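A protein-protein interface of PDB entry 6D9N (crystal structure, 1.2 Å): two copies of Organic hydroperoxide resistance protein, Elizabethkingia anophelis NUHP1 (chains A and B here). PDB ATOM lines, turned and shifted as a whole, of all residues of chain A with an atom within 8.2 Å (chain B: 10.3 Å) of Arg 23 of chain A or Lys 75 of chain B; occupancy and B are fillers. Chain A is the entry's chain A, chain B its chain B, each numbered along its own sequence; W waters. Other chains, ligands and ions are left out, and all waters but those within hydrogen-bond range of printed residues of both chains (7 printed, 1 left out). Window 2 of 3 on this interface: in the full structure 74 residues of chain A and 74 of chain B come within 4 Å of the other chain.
Printed residues of chain B within 4 Å of Thr 20 of chain A: Glu 83 and Thr 84.
Gly 21 of chain A touches just one residue of chain B: Glu 83 (3.0 Å).
Of chain B, only Glu 83 comes within 4 Å of Gly 22 of chain A.
Of chain B, only Lys 75 (3.4 Å) comes within 4 Å of Arg 23 of chain A.
Asn 24 of chain A touches none of the printed residues of chain B.
No residue of chain B comes within 4 Å of Gly 25 of chain A.
Printed residues of chain B within 4 Å of Tyr 40 of chain A: Ser 68.
Lys 75 of chain B touches just one residue of chain A: Arg 23 (3.4 Å).
No residue of chain A comes within 4 Å of Ser 76 of chain B.
The nearest residue of chain B that does not touch Arg 23 of chain A is Asn 71 of chain B (5.9 Å).
The nearest printed residue of chain A that does not touch Lys 75 of chain B is Tyr 40 of chain A (6.9 Å).
Hydrophobic or aromatic side chains of chain A that line the printed part of chain B: Tyr 40.
Among the printed residues, 6 pairs touch across the chains.
Among the printed residues, no Asp or Glu carboxylate lies within 4 Å of a Lys or Arg side-chain nitrogen of the other chain.
Water W5 bridges OH of Tyr 40 of chain A and O of Ser 68 of chain B.
Water W1 bridges the side-chain carboxylate of Glu 83 of chain B (2.7 Å) and the side-chain hydroxyl of Thr 20 of chain A (2.9 Å).
Water W4 bridges the side-chain carboxylate of Asp 67 of chain B (2.8 Å) and the backbone carbonyl oxygen of Thr 20 of chain A (3.0 Å).
Water W7 lies within hydrogen-bond range of the side-chain carboxylate of Asp 67 of chain B (2.8 Å), the backbone carbonyl oxygen of Thr 84 of chain B (2.8 Å), the backbone NH of Gly 22 of chain A (2.9 Å) and the backbone NH of Gly 21 of chain A (3.4 Å).
Water W2 lies within hydrogen-bond range of O of Gly 22 of chain A (2.9 Å), OD2 of Asp 67 of chain B (3.1 Å) and ND2 of Asn 71 of chain B (3.4 Å).
Water W3 bridges NZ of Lys 75 of chain B (3.3 Å) and NH1 of Arg 23 of chain A (3.4 Å).
The guanidinium group (NH2) of Arg 23 of chain A sits close to the side-chain amino group (NZ) of Lys 75 of chain B.
OG1 of Thr 20 of chain A is in hydrogen-bond range of O of Thr 84 of chain B.
The side-chain hydroxyl (OG1) of Thr 20 of chain A lies within hydrogen-bond range of the side-chain carboxylate (OE2) of Glu 83 of chain B (3.0 Å).
N of Gly 21 of chain A lies within hydrogen-bond range of OE2 of Glu 83 of chain B, 3.0 Å away.
ND2 of Asn 71 of chain B is in hydrogen-bond range of OG1 of Thr 84 of chain B, 2.8 Å away.
O of Thr 20 of chain A lies within hydrogen-bond range of N of His 26 of chain A, 2.9 Å away.
OG1 of Thr 84 of chain B is in hydrogen-bond range of OD1 of Asp 67 of chain B (2.6 Å).
O of Lys 75 of chain B lies within hydrogen-bond range of NZ of Lys 78 of chain B, 2.8 Å away.
N of Gly 22 of chain A touches CD of Glu 83 of chain B, at 3.8 Å.
Ser 68 of chain B touches Tyr 40 of chain A (OG to CE1, 3.6 Å).
No position is printed for both chains.
Of the 6 pairs that touch across the chains among the printed residues, none has its exchanged pair printed and touching as well.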
ATOM      1  N   THR A  20     -17.644 -26.876  20.909  1.00  0.00           N
ATOM      2  CA  THR A  20     -16.834 -26.001  20.069  1.00  0.00           C
ATOM      3  C   THR A  20     -15.850 -26.894  19.315  1.00  0.00           C
ATOM      4  O   THR A  20     -16.118 -28.089  19.141  1.00  0.00           O
ATOM      5  CB  THR A  20     -16.224 -24.873  20.911  1.00  0.00           C
ATOM      6  OG1 THR A  20     -15.578 -23.940  20.049  1.00  0.00           O
ATOM      7  CG2 THR A  20     -15.221 -25.397  21.920  1.00  0.00           C
ATOM      8  N   GLY A  21     -14.772 -26.305  18.764  1.00  0.00           N
ATOM      9  CA  GLY A  21     -13.716 -27.079  18.147  1.00  0.00           C
ATOM     10  C   GLY A  21     -13.693 -27.115  16.631  1.00  0.00           C
ATOM     11  O   GLY A  21     -12.753 -27.692  16.067  1.00  0.00           O
ATOM     12  N   GLY A  22     -14.713 -26.579  15.957  1.00  0.00           N
ATOM     13  CA  GLY A  22     -14.683 -26.590  14.504  1.00  0.00           C
ATOM     14  C   GLY A  22     -14.724 -28.010  13.964  1.00  0.00           C
ATOM     15  O   GLY A  22     -15.594 -28.827  14.320  1.00  0.00           O
ATOM     16  N   ARG A  23     -13.749 -28.334  13.104  1.00  0.00           N
ATOM     17  CA  ARG A  23     -13.646 -29.667  12.512  1.00  0.00           C
ATOM     18  C   ARG A  23     -13.198 -30.711  13.522  1.00  0.00           C
ATOM     19  O   ARG A  23     -13.331 -31.914  13.254  1.00  0.00           O
ATOM     20  CB  ARG A  23     -12.708 -29.659  11.296  1.00  0.00           C
ATOM     21  CG  ARG A  23     -13.288 -28.879  10.112  1.00  0.00           C
ATOM     22  CD  ARG A  23     -12.453 -29.014   8.819  1.00  0.00           C
ATOM     23  NE  ARG A  23     -13.278 -28.689   7.651  1.00  0.00           N
ATOM     24  CZ  ARG A  23     -13.343 -27.492   7.066  1.00  0.00           C
ATOM     25  NH1 ARG A  23     -14.144 -27.312   6.017  1.00  0.00           N
ATOM     26  NH2 ARG A  23     -12.609 -26.478   7.512  1.00  0.00           N
ATOM     27  N   ASN A  24     -12.633 -30.284  14.640  1.00  0.00           N
ATOM     28  CA  ASN A  24     -12.251 -31.187  15.719  1.00  0.00           C
ATOM     29  C   ASN A  24     -13.204 -30.957  16.884  1.00  0.00           C
ATOM     30  O   ASN A  24     -12.829 -30.432  17.937  1.00  0.00           O
ATOM     31  CB  ASN A  24     -10.804 -30.941  16.130  1.00  0.00           C
ATOM     32  CG  ASN A  24      -9.817 -31.301  15.034  1.00  0.00           C
ATOM     33  OD1 ASN A  24     -10.070 -32.187  14.213  1.00  0.00           O
ATOM     34  ND2 ASN A  24      -8.686 -30.611  15.010  1.00  0.00           N
ATOM     35  N   GLY A  25     -14.456 -31.351  16.663  1.00  0.00           N
ATOM     36  CA  GLY A  25     -15.509 -31.024  17.619  1.00  0.00           C
ATOM     37  C   GLY A  25     -15.210 -31.579  19.003  1.00  0.00           C
ATOM     38  O   GLY A  25     -14.667 -32.676  19.162  1.00  0.00           O
ATOM     39  N   HIS A  26     -15.588 -30.802  20.012  1.00  0.00           N
ATOM     40  CA  HIS A  26     -15.358 -31.090  21.421  1.00  0.00           C
ATOM     41  C   HIS A  26     -16.591 -30.646  22.199  1.00  0.00           C
ATOM     42  O   HIS A  26     -17.110 -29.562  21.912  1.00  0.00           O
ATOM     43  CB  HIS A  26     -14.170 -30.217  21.867  1.00  0.00           C
ATOM     44  CG  HIS A  26     -13.629 -30.583  23.209  1.00  0.00           C
ATOM     45  ND1 HIS A  26     -12.722 -31.605  23.388  1.00  0.00           N
ATOM     46  CD2 HIS A  26     -13.881 -30.080  24.440  1.00  0.00           C
ATOM     47  CE1 HIS A  26     -12.429 -31.707  24.673  1.00  0.00           C
ATOM     48  NE2 HIS A  26     -13.113 -30.789  25.330  1.00  0.00           N
ATOM     49  N   GLU A  37     -14.784 -35.873  22.457  1.00  0.00           N
ATOM     50  CA  GLU A  37     -14.710 -35.361  21.109  1.00  0.00           C
ATOM     51  C   GLU A  37     -15.841 -35.939  20.267  1.00  0.00           C
ATOM     52  O   GLU A  37     -16.331 -37.055  20.501  1.00  0.00           O
ATOM     53  CB  GLU A  37     -13.354 -35.677  20.480  1.00  0.00           C
ATOM     54  CG  GLU A  37     -12.181 -34.978  21.166  1.00  0.00           C
ATOM     55  CD  GLU A  37     -10.902 -35.176  20.401  1.00  0.00           C
ATOM     56  OE1 GLU A  37     -10.514 -34.283  19.607  1.00  0.00           O
ATOM     57  OE2 GLU A  37     -10.302 -36.256  20.555  1.00  0.00           O
ATOM     58  N   VAL A  38     -16.278 -35.147  19.287  1.00  0.00           N
ATOM     59  CA  VAL A  38     -17.302 -35.573  18.344  1.00  0.00           C
ATOM     60  C   VAL A  38     -16.773 -35.382  16.929  1.00  0.00           C
ATOM     61  O   VAL A  38     -16.000 -34.445  16.656  1.00  0.00           O
ATOM     62  CB  VAL A  38     -18.638 -34.833  18.539  1.00  0.00           C
ATOM     63  CG1 VAL A  38     -19.284 -35.248  19.863  1.00  0.00           C
ATOM     64  CG2 VAL A  38     -18.477 -33.326  18.435  1.00  0.00           C
ATOM     65  N   ARG A  39     -17.157 -36.289  16.036  1.00  0.00           N
ATOM     66  CA  ARG A  39     -16.804 -36.198  14.628  1.00  0.00           C
ATOM     67  C   ARG A  39     -17.969 -36.792  13.855  1.00  0.00           C
ATOM     68  O   ARG A  39     -18.767 -37.566  14.396  1.00  0.00           O
ATOM     69  CB  ARG A  39     -15.555 -37.042  14.290  1.00  0.00           C
ATOM     70  CG  ARG A  39     -14.286 -36.696  15.044  1.00  0.00           C
ATOM     71  CD  ARG A  39     -13.639 -35.404  14.571  1.00  0.00           C
ATOM     72  NE  ARG A  39     -12.322 -35.237  15.198  1.00  0.00           N
ATOM     73  CZ  ARG A  39     -12.076 -34.678  16.391  1.00  0.00           C
ATOM     74  NH1 ARG A  39     -13.051 -34.218  17.158  1.00  0.00           N
ATOM     75  NH2 ARG A  39     -10.816 -34.585  16.833  1.00  0.00           N
ATOM     76  N   TYR A  40     -18.066 -36.489  12.573  1.00  0.00           N
ATOM     77  CA  TYR A  40     -19.039 -37.178  11.727  1.00  0.00           C
ATOM     78  C   TYR A  40     -18.704 -38.663  11.641  1.00  0.00           C
ATOM     79  O   TYR A  40     -17.531 -39.020  11.422  1.00  0.00           O
ATOM     80  CB  TYR A  40     -18.952 -36.668  10.288  1.00  0.00           C
ATOM     81  CG  TYR A  40     -19.326 -35.218   9.993  1.00  0.00           C
ATOM     82  CD1 TYR A  40     -19.959 -34.402  10.929  1.00  0.00           C
ATOM     83  CD2 TYR A  40     -19.022 -34.661   8.742  1.00  0.00           C
ATOM     84  CE1 TYR A  40     -20.295 -33.066  10.615  1.00  0.00           C
ATOM     85  CE2 TYR A  40     -19.345 -33.354   8.422  1.00  0.00           C
ATOM     86  CZ  TYR A  40     -19.985 -32.549   9.348  1.00  0.00           C
ATOM     87  OH  TYR A  40     -20.287 -31.244   8.982  1.00  0.00           O
ATOM     88  N   ASP B  67     -24.122 -26.866  17.023  1.00  0.00           N
ATOM     89  CA  ASP B  67     -22.848 -26.393  16.495  1.00  0.00           C
ATOM     90  C   ASP B  67     -22.505 -27.066  15.174  1.00  0.00           C
ATOM     91  O   ASP B  67     -22.008 -26.398  14.248  1.00  0.00           O
ATOM     92  CB  ASP B  67     -21.716 -26.624  17.499  1.00  0.00           C
ATOM     93  CG  ASP B  67     -20.492 -25.789  17.136  1.00  0.00           C
ATOM     94  OD1 ASP B  67     -20.634 -24.550  17.078  1.00  0.00           O
ATOM     95  OD2 ASP B  67     -19.417 -26.365  16.855  1.00  0.00           O
ATOM     96  N   SER B  68     -22.797 -28.363  15.032  1.00  0.00           N
ATOM     97  CA  SER B  68     -22.539 -29.049  13.768  1.00  0.00           C
ATOM     98  C   SER B  68     -23.391 -28.462  12.643  1.00  0.00           C
ATOM     99  O   SER B  68     -22.888 -28.166  11.546  1.00  0.00           O
ATOM    100  CB  SER B  68     -22.838 -30.536  13.939  1.00  0.00           C
ATOM    101  OG  SER B  68     -22.612 -31.200  12.715  1.00  0.00           O
ATOM    102  N   ALA B  69     -24.678 -28.237  12.908  1.00  0.00           N
ATOM    103  CA  ALA B  69     -25.574 -27.662  11.907  1.00  0.00           C
ATOM    104  C   ALA B  69     -25.134 -26.253  11.546  1.00  0.00           C
ATOM    105  O   ALA B  69     -25.114 -25.878  10.370  1.00  0.00           O
ATOM    106  CB  ALA B  69     -27.005 -27.646  12.461  1.00  0.00           C
ATOM    107  N   LEU B  70     -24.742 -25.454  12.547  1.00  0.00           N
ATOM    108  CA  LEU B  70     -24.264 -24.095  12.313  1.00  0.00           C
ATOM    109  C   LEU B  70     -23.039 -24.098  11.406  1.00  0.00           C
ATOM    110  O   LEU B  70     -22.933 -23.278  10.489  1.00  0.00           O
ATOM    111  CB  LEU B  70     -23.983 -23.480  13.680  1.00  0.00           C
ATOM    112  CG  LEU B  70     -23.464 -22.043  13.640  1.00  0.00           C
ATOM    113  CD1 LEU B  70     -24.446 -21.116  12.948  1.00  0.00           C
ATOM    114  CD2 LEU B  70     -23.211 -21.611  15.072  1.00  0.00           C
ATOM    115  N   ASN B  71     -22.098 -25.015  11.646  1.00  0.00           N
ATOM    116  CA  ASN B  71     -20.910 -25.072  10.801  1.00  0.00           C
ATOM    117  C   ASN B  71     -21.244 -25.541   9.400  1.00  0.00           C
ATOM    118  O   ASN B  71     -20.641 -25.045   8.430  1.00  0.00           O
ATOM    119  CB  ASN B  71     -19.815 -25.869  11.494  1.00  0.00           C
ATOM    120  CG  ASN B  71     -19.097 -25.026  12.502  1.00  0.00           C
ATOM    121  OD1 ASN B  71     -18.055 -24.447  12.199  1.00  0.00           O
ATOM    122  ND2 ASN B  71     -19.699 -24.819  13.650  1.00  0.00           N
ATOM    123  N   LEU B  72     -22.216 -26.440   9.240  1.00  0.00           N
ATOM    124  CA  LEU B  72     -22.623 -26.815   7.887  1.00  0.00           C
ATOM    125  C   LEU B  72     -23.198 -25.616   7.138  1.00  0.00           C
ATOM    126  O   LEU B  72     -22.907 -25.397   5.946  1.00  0.00           O
ATOM    127  CB  LEU B  72     -23.626 -27.962   7.974  1.00  0.00           C
ATOM    128  CG  LEU B  72     -24.072 -28.501   6.623  1.00  0.00           C
ATOM    129  CD1 LEU B  72     -22.886 -28.953   5.720  1.00  0.00           C
ATOM    130  CD2 LEU B  72     -25.054 -29.656   6.885  1.00  0.00           C
ATOM    131  N   VAL B  73     -24.037 -24.840   7.817  1.00  0.00           N
ATOM    132  CA  VAL B  73     -24.633 -23.652   7.206  1.00  0.00           C
ATOM    133  C   VAL B  73     -23.549 -22.639   6.828  1.00  0.00           C
ATOM    134  O   VAL B  73     -23.571 -22.060   5.741  1.00  0.00           O
ATOM    135  CB  VAL B  73     -25.681 -23.059   8.168  1.00  0.00           C
ATOM    136  CG1 VAL B  73     -26.134 -21.650   7.744  1.00  0.00           C
ATOM    137  CG2 VAL B  73     -26.876 -23.985   8.290  1.00  0.00           C
ATOM    138  N   ILE B  74     -22.596 -22.398   7.728  1.00  0.00           N
ATOM    139  CA  ILE B  74     -21.489 -21.474   7.448  1.00  0.00           C
ATOM    140  C   ILE B  74     -20.698 -21.919   6.219  1.00  0.00           C
ATOM    141  O   ILE B  74     -20.388 -21.109   5.327  1.00  0.00           O
ATOM    142  CB  ILE B  74     -20.598 -21.350   8.699  1.00  0.00           C
ATOM    143  CG1 ILE B  74     -21.316 -20.544   9.775  1.00  0.00           C
ATOM    144  CG2 ILE B  74     -19.266 -20.728   8.319  1.00  0.00           C
ATOM    145  CD1 ILE B  74     -20.616 -20.616  11.150  1.00  0.00           C
ATOM    146  N   LYS B  75     -20.362 -23.216   6.146  1.00  0.00           N
ATOM    147  CA  LYS B  75     -19.563 -23.686   5.022  1.00  0.00           C
ATOM    148  C   LYS B  75     -20.359 -23.632   3.730  1.00  0.00           C
ATOM    149  O   LYS B  75     -19.808 -23.286   2.667  1.00  0.00           O
ATOM    150  CB  LYS B  75     -19.078 -25.115   5.290  1.00  0.00           C
ATOM    151  CG  LYS B  75     -18.037 -25.244   6.418  1.00  0.00           C
ATOM    152  CD  LYS B  75     -16.704 -24.537   6.099  1.00  0.00           C
ATOM    153  CE  LYS B  75     -15.702 -24.617   7.286  1.00  0.00           C
ATOM    154  NZ  LYS B  75     -14.544 -23.676   7.046  1.00  0.00           N
ATOM    155  N   SER B  76     -21.656 -23.898   3.799  1.00  0.00           N
ATOM    156  CA  SER B  76     -22.483 -23.827   2.600  1.00  0.00           C
ATOM    157  C   SER B  76     -22.549 -22.405   2.059  1.00  0.00           C
ATOM    158  O   SER B  76     -22.657 -22.203   0.841  1.00  0.00           O
ATOM    159  CB  SER B  76     -23.877 -24.402   2.892  1.00  0.00           C
ATOM    160  OG  SER B  76     -23.785 -25.796   3.211  1.00  0.00           O
ATOM    161  N   ALA B  77     -22.459 -21.411   2.945  1.00  0.00           N
ATOM    162  CA  ALA B  77     -22.525 -19.999   2.575  1.00  0.00           C
ATOM    163  C   ALA B  77     -21.169 -19.429   2.178  1.00  0.00           C
ATOM    164  O   ALA B  77     -21.107 -18.305   1.666  1.00  0.00           O
ATOM    165  CB  ALA B  77     -23.082 -19.180   3.750  1.00  0.00           C
ATOM    166  N   LYS B  78     -20.092 -20.157   2.404  1.00  0.00           N
ATOM    167  CA  LYS B  78     -18.751 -19.676   2.086  1.00  0.00           C
ATOM    168  C   LYS B  78     -18.426 -18.374   2.833  1.00  0.00           C
ATOM    169  O   LYS B  78     -17.690 -17.524   2.327  1.00  0.00           O
ATOM    170  CB  LYS B  78     -18.493 -19.637   0.568  1.00  0.00           C
ATOM    171  CG  LYS B  78     -18.275 -21.087   0.052  1.00  0.00           C
ATOM    172  CD  LYS B  78     -16.875 -21.631   0.569  1.00  0.00           C
ATOM    173  CE  LYS B  78     -16.711 -23.156   0.733  1.00  0.00           C
ATOM    174  NZ  LYS B  78     -17.161 -23.701   2.044  1.00  0.00           N
ATOM    175  N   ILE B  79     -18.936 -18.202   4.080  1.00  0.00           N
ATOM    176  CA  ILE B  79     -18.711 -17.005   4.905  1.00  0.00           C
ATOM    177  C   ILE B  79     -17.544 -17.277   5.853  1.00  0.00           C
ATOM    178  O   ILE B  79     -17.510 -18.332   6.521  1.00  0.00           O
ATOM    179  CB  ILE B  79     -19.991 -16.590   5.670  1.00  0.00           C
ATOM    180  CG1 ILE B  79     -19.751 -15.322   6.526  1.00  0.00           C
ATOM    181  CG2 ILE B  79     -20.490 -17.713   6.527  1.00  0.00           C
ATOM    182  CD1 ILE B  79     -21.038 -14.603   7.007  1.00  0.00           C
ATOM    183  N   LYS B  80     -16.609 -16.331   5.953  1.00  0.00           N
ATOM    184  CA  LYS B  80     -15.501 -16.416   6.897  1.00  0.00           C
ATOM    185  C   LYS B  80     -15.969 -16.092   8.309  1.00  0.00           C
ATOM    186  O   LYS B  80     -16.568 -15.036   8.544  1.00  0.00           O
ATOM    187  CB  LYS B  80     -14.421 -15.399   6.513  1.00  0.00           C
ATOM    188  CG  LYS B  80     -13.201 -15.420   7.397  1.00  0.00           C
ATOM    189  CD  LYS B  80     -12.210 -14.309   7.007  1.00  0.00           C
ATOM    190  CE  LYS B  80     -10.997 -14.306   7.910  1.00  0.00           C
ATOM    191  NZ  LYS B  80     -10.076 -13.171   7.570  1.00  0.00           N
ATOM    192  N   THR B  81     -15.720 -17.010   9.244  1.00  0.00           N
ATOM    193  CA  THR B  81     -16.026 -16.764  10.649  1.00  0.00           C
ATOM    194  C   THR B  81     -14.894 -17.302  11.493  1.00  0.00           C
ATOM    195  O   THR B  81     -14.098 -18.133  11.033  1.00  0.00           O
ATOM    196  CB  THR B  81     -17.323 -17.457  11.128  1.00  0.00           C
ATOM    197  OG1 THR B  81     -17.103 -18.838  11.436  1.00  0.00           O
ATOM    198  CG2 THR B  81     -18.404 -17.384  10.115  1.00  0.00           C
ATOM    199  N   GLY B  82     -14.858 -16.894  12.756  1.00  0.00           N
ATOM    200  CA  GLY B  82     -14.022 -17.583  13.707  1.00  0.00           C
ATOM    201  C   GLY B  82     -14.657 -18.885  14.171  1.00  0.00           C
ATOM    202  O   GLY B  82     -15.762 -19.245  13.787  1.00  0.00           O
ATOM    203  N   GLU B  83     -13.966 -19.580  15.061  1.00  0.00           N
ATOM    204  CA  GLU B  83     -14.496 -20.856  15.548  1.00  0.00           C
ATOM    205  C   GLU B  83     -15.726 -20.604  16.419  1.00  0.00           C
ATOM    206  O   GLU B  83     -15.685 -19.759  17.323  1.00  0.00           O
ATOM    207  CB  GLU B  83     -13.418 -21.601  16.324  1.00  0.00           C
ATOM    208  CG  GLU B  83     -13.888 -22.981  16.835  1.00  0.00           C
ATOM    209  CD  GLU B  83     -12.763 -23.752  17.483  1.00  0.00           C
ATOM    210  OE1 GLU B  83     -11.795 -24.119  16.773  1.00  0.00           O
ATOM    211  OE2 GLU B  83     -12.871 -23.995  18.695  1.00  0.00           O
ATOM    212  N   THR B  84     -16.823 -21.289  16.100  1.00  0.00           N
ATOM    213  CA  THR B  84     -18.076 -21.062  16.819  1.00  0.00           C
ATOM    214  C   THR B  84     -18.106 -21.830  18.136  1.00  0.00           C
ATOM    215  O   THR B  84     -17.367 -22.812  18.344  1.00  0.00           O
ATOM    216  CB  THR B  84     -19.274 -21.503  15.956  1.00  0.00           C
ATOM    217  OG1 THR B  84     -19.163 -22.898  15.665  1.00  0.00           O
ATOM    218  CG2 THR B  84     -19.336 -20.734  14.662  1.00  0.00           C
ATOM    219  N   ILE B 110     -20.614 -16.546  17.244  1.00  0.00           N
ATOM    220  CA  ILE B 110     -20.002 -16.628  15.910  1.00  0.00           C
ATOM    221  C   ILE B 110     -19.054 -15.447  15.768  1.00  0.00           C
ATOM    222  O   ILE B 110     -19.502 -14.322  15.460  1.00  0.00           O
ATOM    223  CB  ILE B 110     -21.065 -16.613  14.794  1.00  0.00           C
ATOM    224  CG1 ILE B 110     -22.158 -17.656  15.044  1.00  0.00           C
ATOM    225  CG2 ILE B 110     -20.386 -16.830  13.429  1.00  0.00           C
ATOM    226  CD1 ILE B 110     -23.371 -17.526  14.104  1.00  0.00           C
ATOM    227  N   VAL B 113     -18.453 -11.971  12.378  1.00  0.00           N
ATOM    228  CA  VAL B 113     -19.561 -11.653  11.493  1.00  0.00           C
ATOM    229  C   VAL B 113     -20.371 -10.519  12.100  1.00  0.00           C
ATOM    230  O   VAL B 113     -20.247 -10.201  13.287  1.00  0.00           O
ATOM    231  CB  VAL B 113     -20.458 -12.878  11.230  1.00  0.00           C
ATOM    232  CG1 VAL B 113     -19.649 -14.025  10.679  1.00  0.00           C
ATOM    233  CG2 VAL B 113     -21.194 -13.332  12.521  1.00  0.00           C
ATOM    234  N   LEU B 121     -27.560 -16.952  10.158  1.00  0.00           N
ATOM    235  CA  LEU B 121     -26.916 -18.248  10.302  1.00  0.00           C
ATOM    236  C   LEU B 121     -27.631 -19.106  11.337  1.00  0.00           C
ATOM    237  O   LEU B 121     -27.889 -20.296  11.085  1.00  0.00           O
ATOM    238  CB  LEU B 121     -25.435 -18.076  10.663  1.00  0.00           C
ATOM    239  CG  LEU B 121     -24.582 -17.475   9.536  1.00  0.00           C
ATOM    240  CD1 LEU B 121     -23.232 -17.038  10.140  1.00  0.00           C
ATOM    241  CD2 LEU B 121     -24.402 -18.478   8.396  1.00  0.00           C
ATOM    242  N   LYS B 124     -31.035 -20.493  10.118  1.00  0.00           N
ATOM    243  CA  LYS B 124     -30.901 -21.676   9.270  1.00  0.00           C
ATOM    244  C   LYS B 124     -30.468 -22.885  10.089  1.00  0.00           C
ATOM    245  O   LYS B 124     -30.990 -23.985   9.876  1.00  0.00           O
ATOM    246  CB  LYS B 124     -29.920 -21.405   8.109  1.00  0.00           C
ATOM    247  CG  LYS B 124     -30.512 -20.512   7.034  1.00  0.00           C
ATOM    248  CD  LYS B 124     -29.517 -20.170   5.948  1.00  0.00           C
ATOM    249  CE  LYS B 124     -30.138 -19.214   4.915  1.00  0.00           C
ATOM    250  NZ  LYS B 124     -29.149 -18.520   4.030  1.00  0.00           N
ATOM    251  N   ALA B 125     -29.490 -22.712  10.984  1.00  0.00           N
ATOM    252  CA  ALA B 125     -29.025 -23.834  11.789  1.00  0.00           C
ATOM    253  C   ALA B 125     -30.157 -24.457  12.589  1.00  0.00           C
ATOM    254  O   ALA B 125     -30.201 -25.675  12.763  1.00  0.00           O
ATOM    255  CB  ALA B 125     -27.922 -23.357  12.714  1.00  0.00           C
HETATM  256  O   HOH W   1     -13.190 -22.389  20.813  1.00  0.00           O
HETATM  257  O   HOH W   2     -18.304 -27.782  14.382  1.00  0.00           O
HETATM  258  O   HOH W   3     -13.471 -24.576   4.070  1.00  0.00           O
HETATM  259  O   HOH W   4     -18.888 -28.757  18.107  1.00  0.00           O
HETATM  260  O   HOH W   5     -20.631 -29.425  10.533  1.00  0.00           O
HETATM  261  O   HOH W   6     -19.234 -28.121   8.530  1.00  0.00           O
HETATM  262  O   HOH W   7     -17.039 -24.993  16.572  1.00  0.00           O
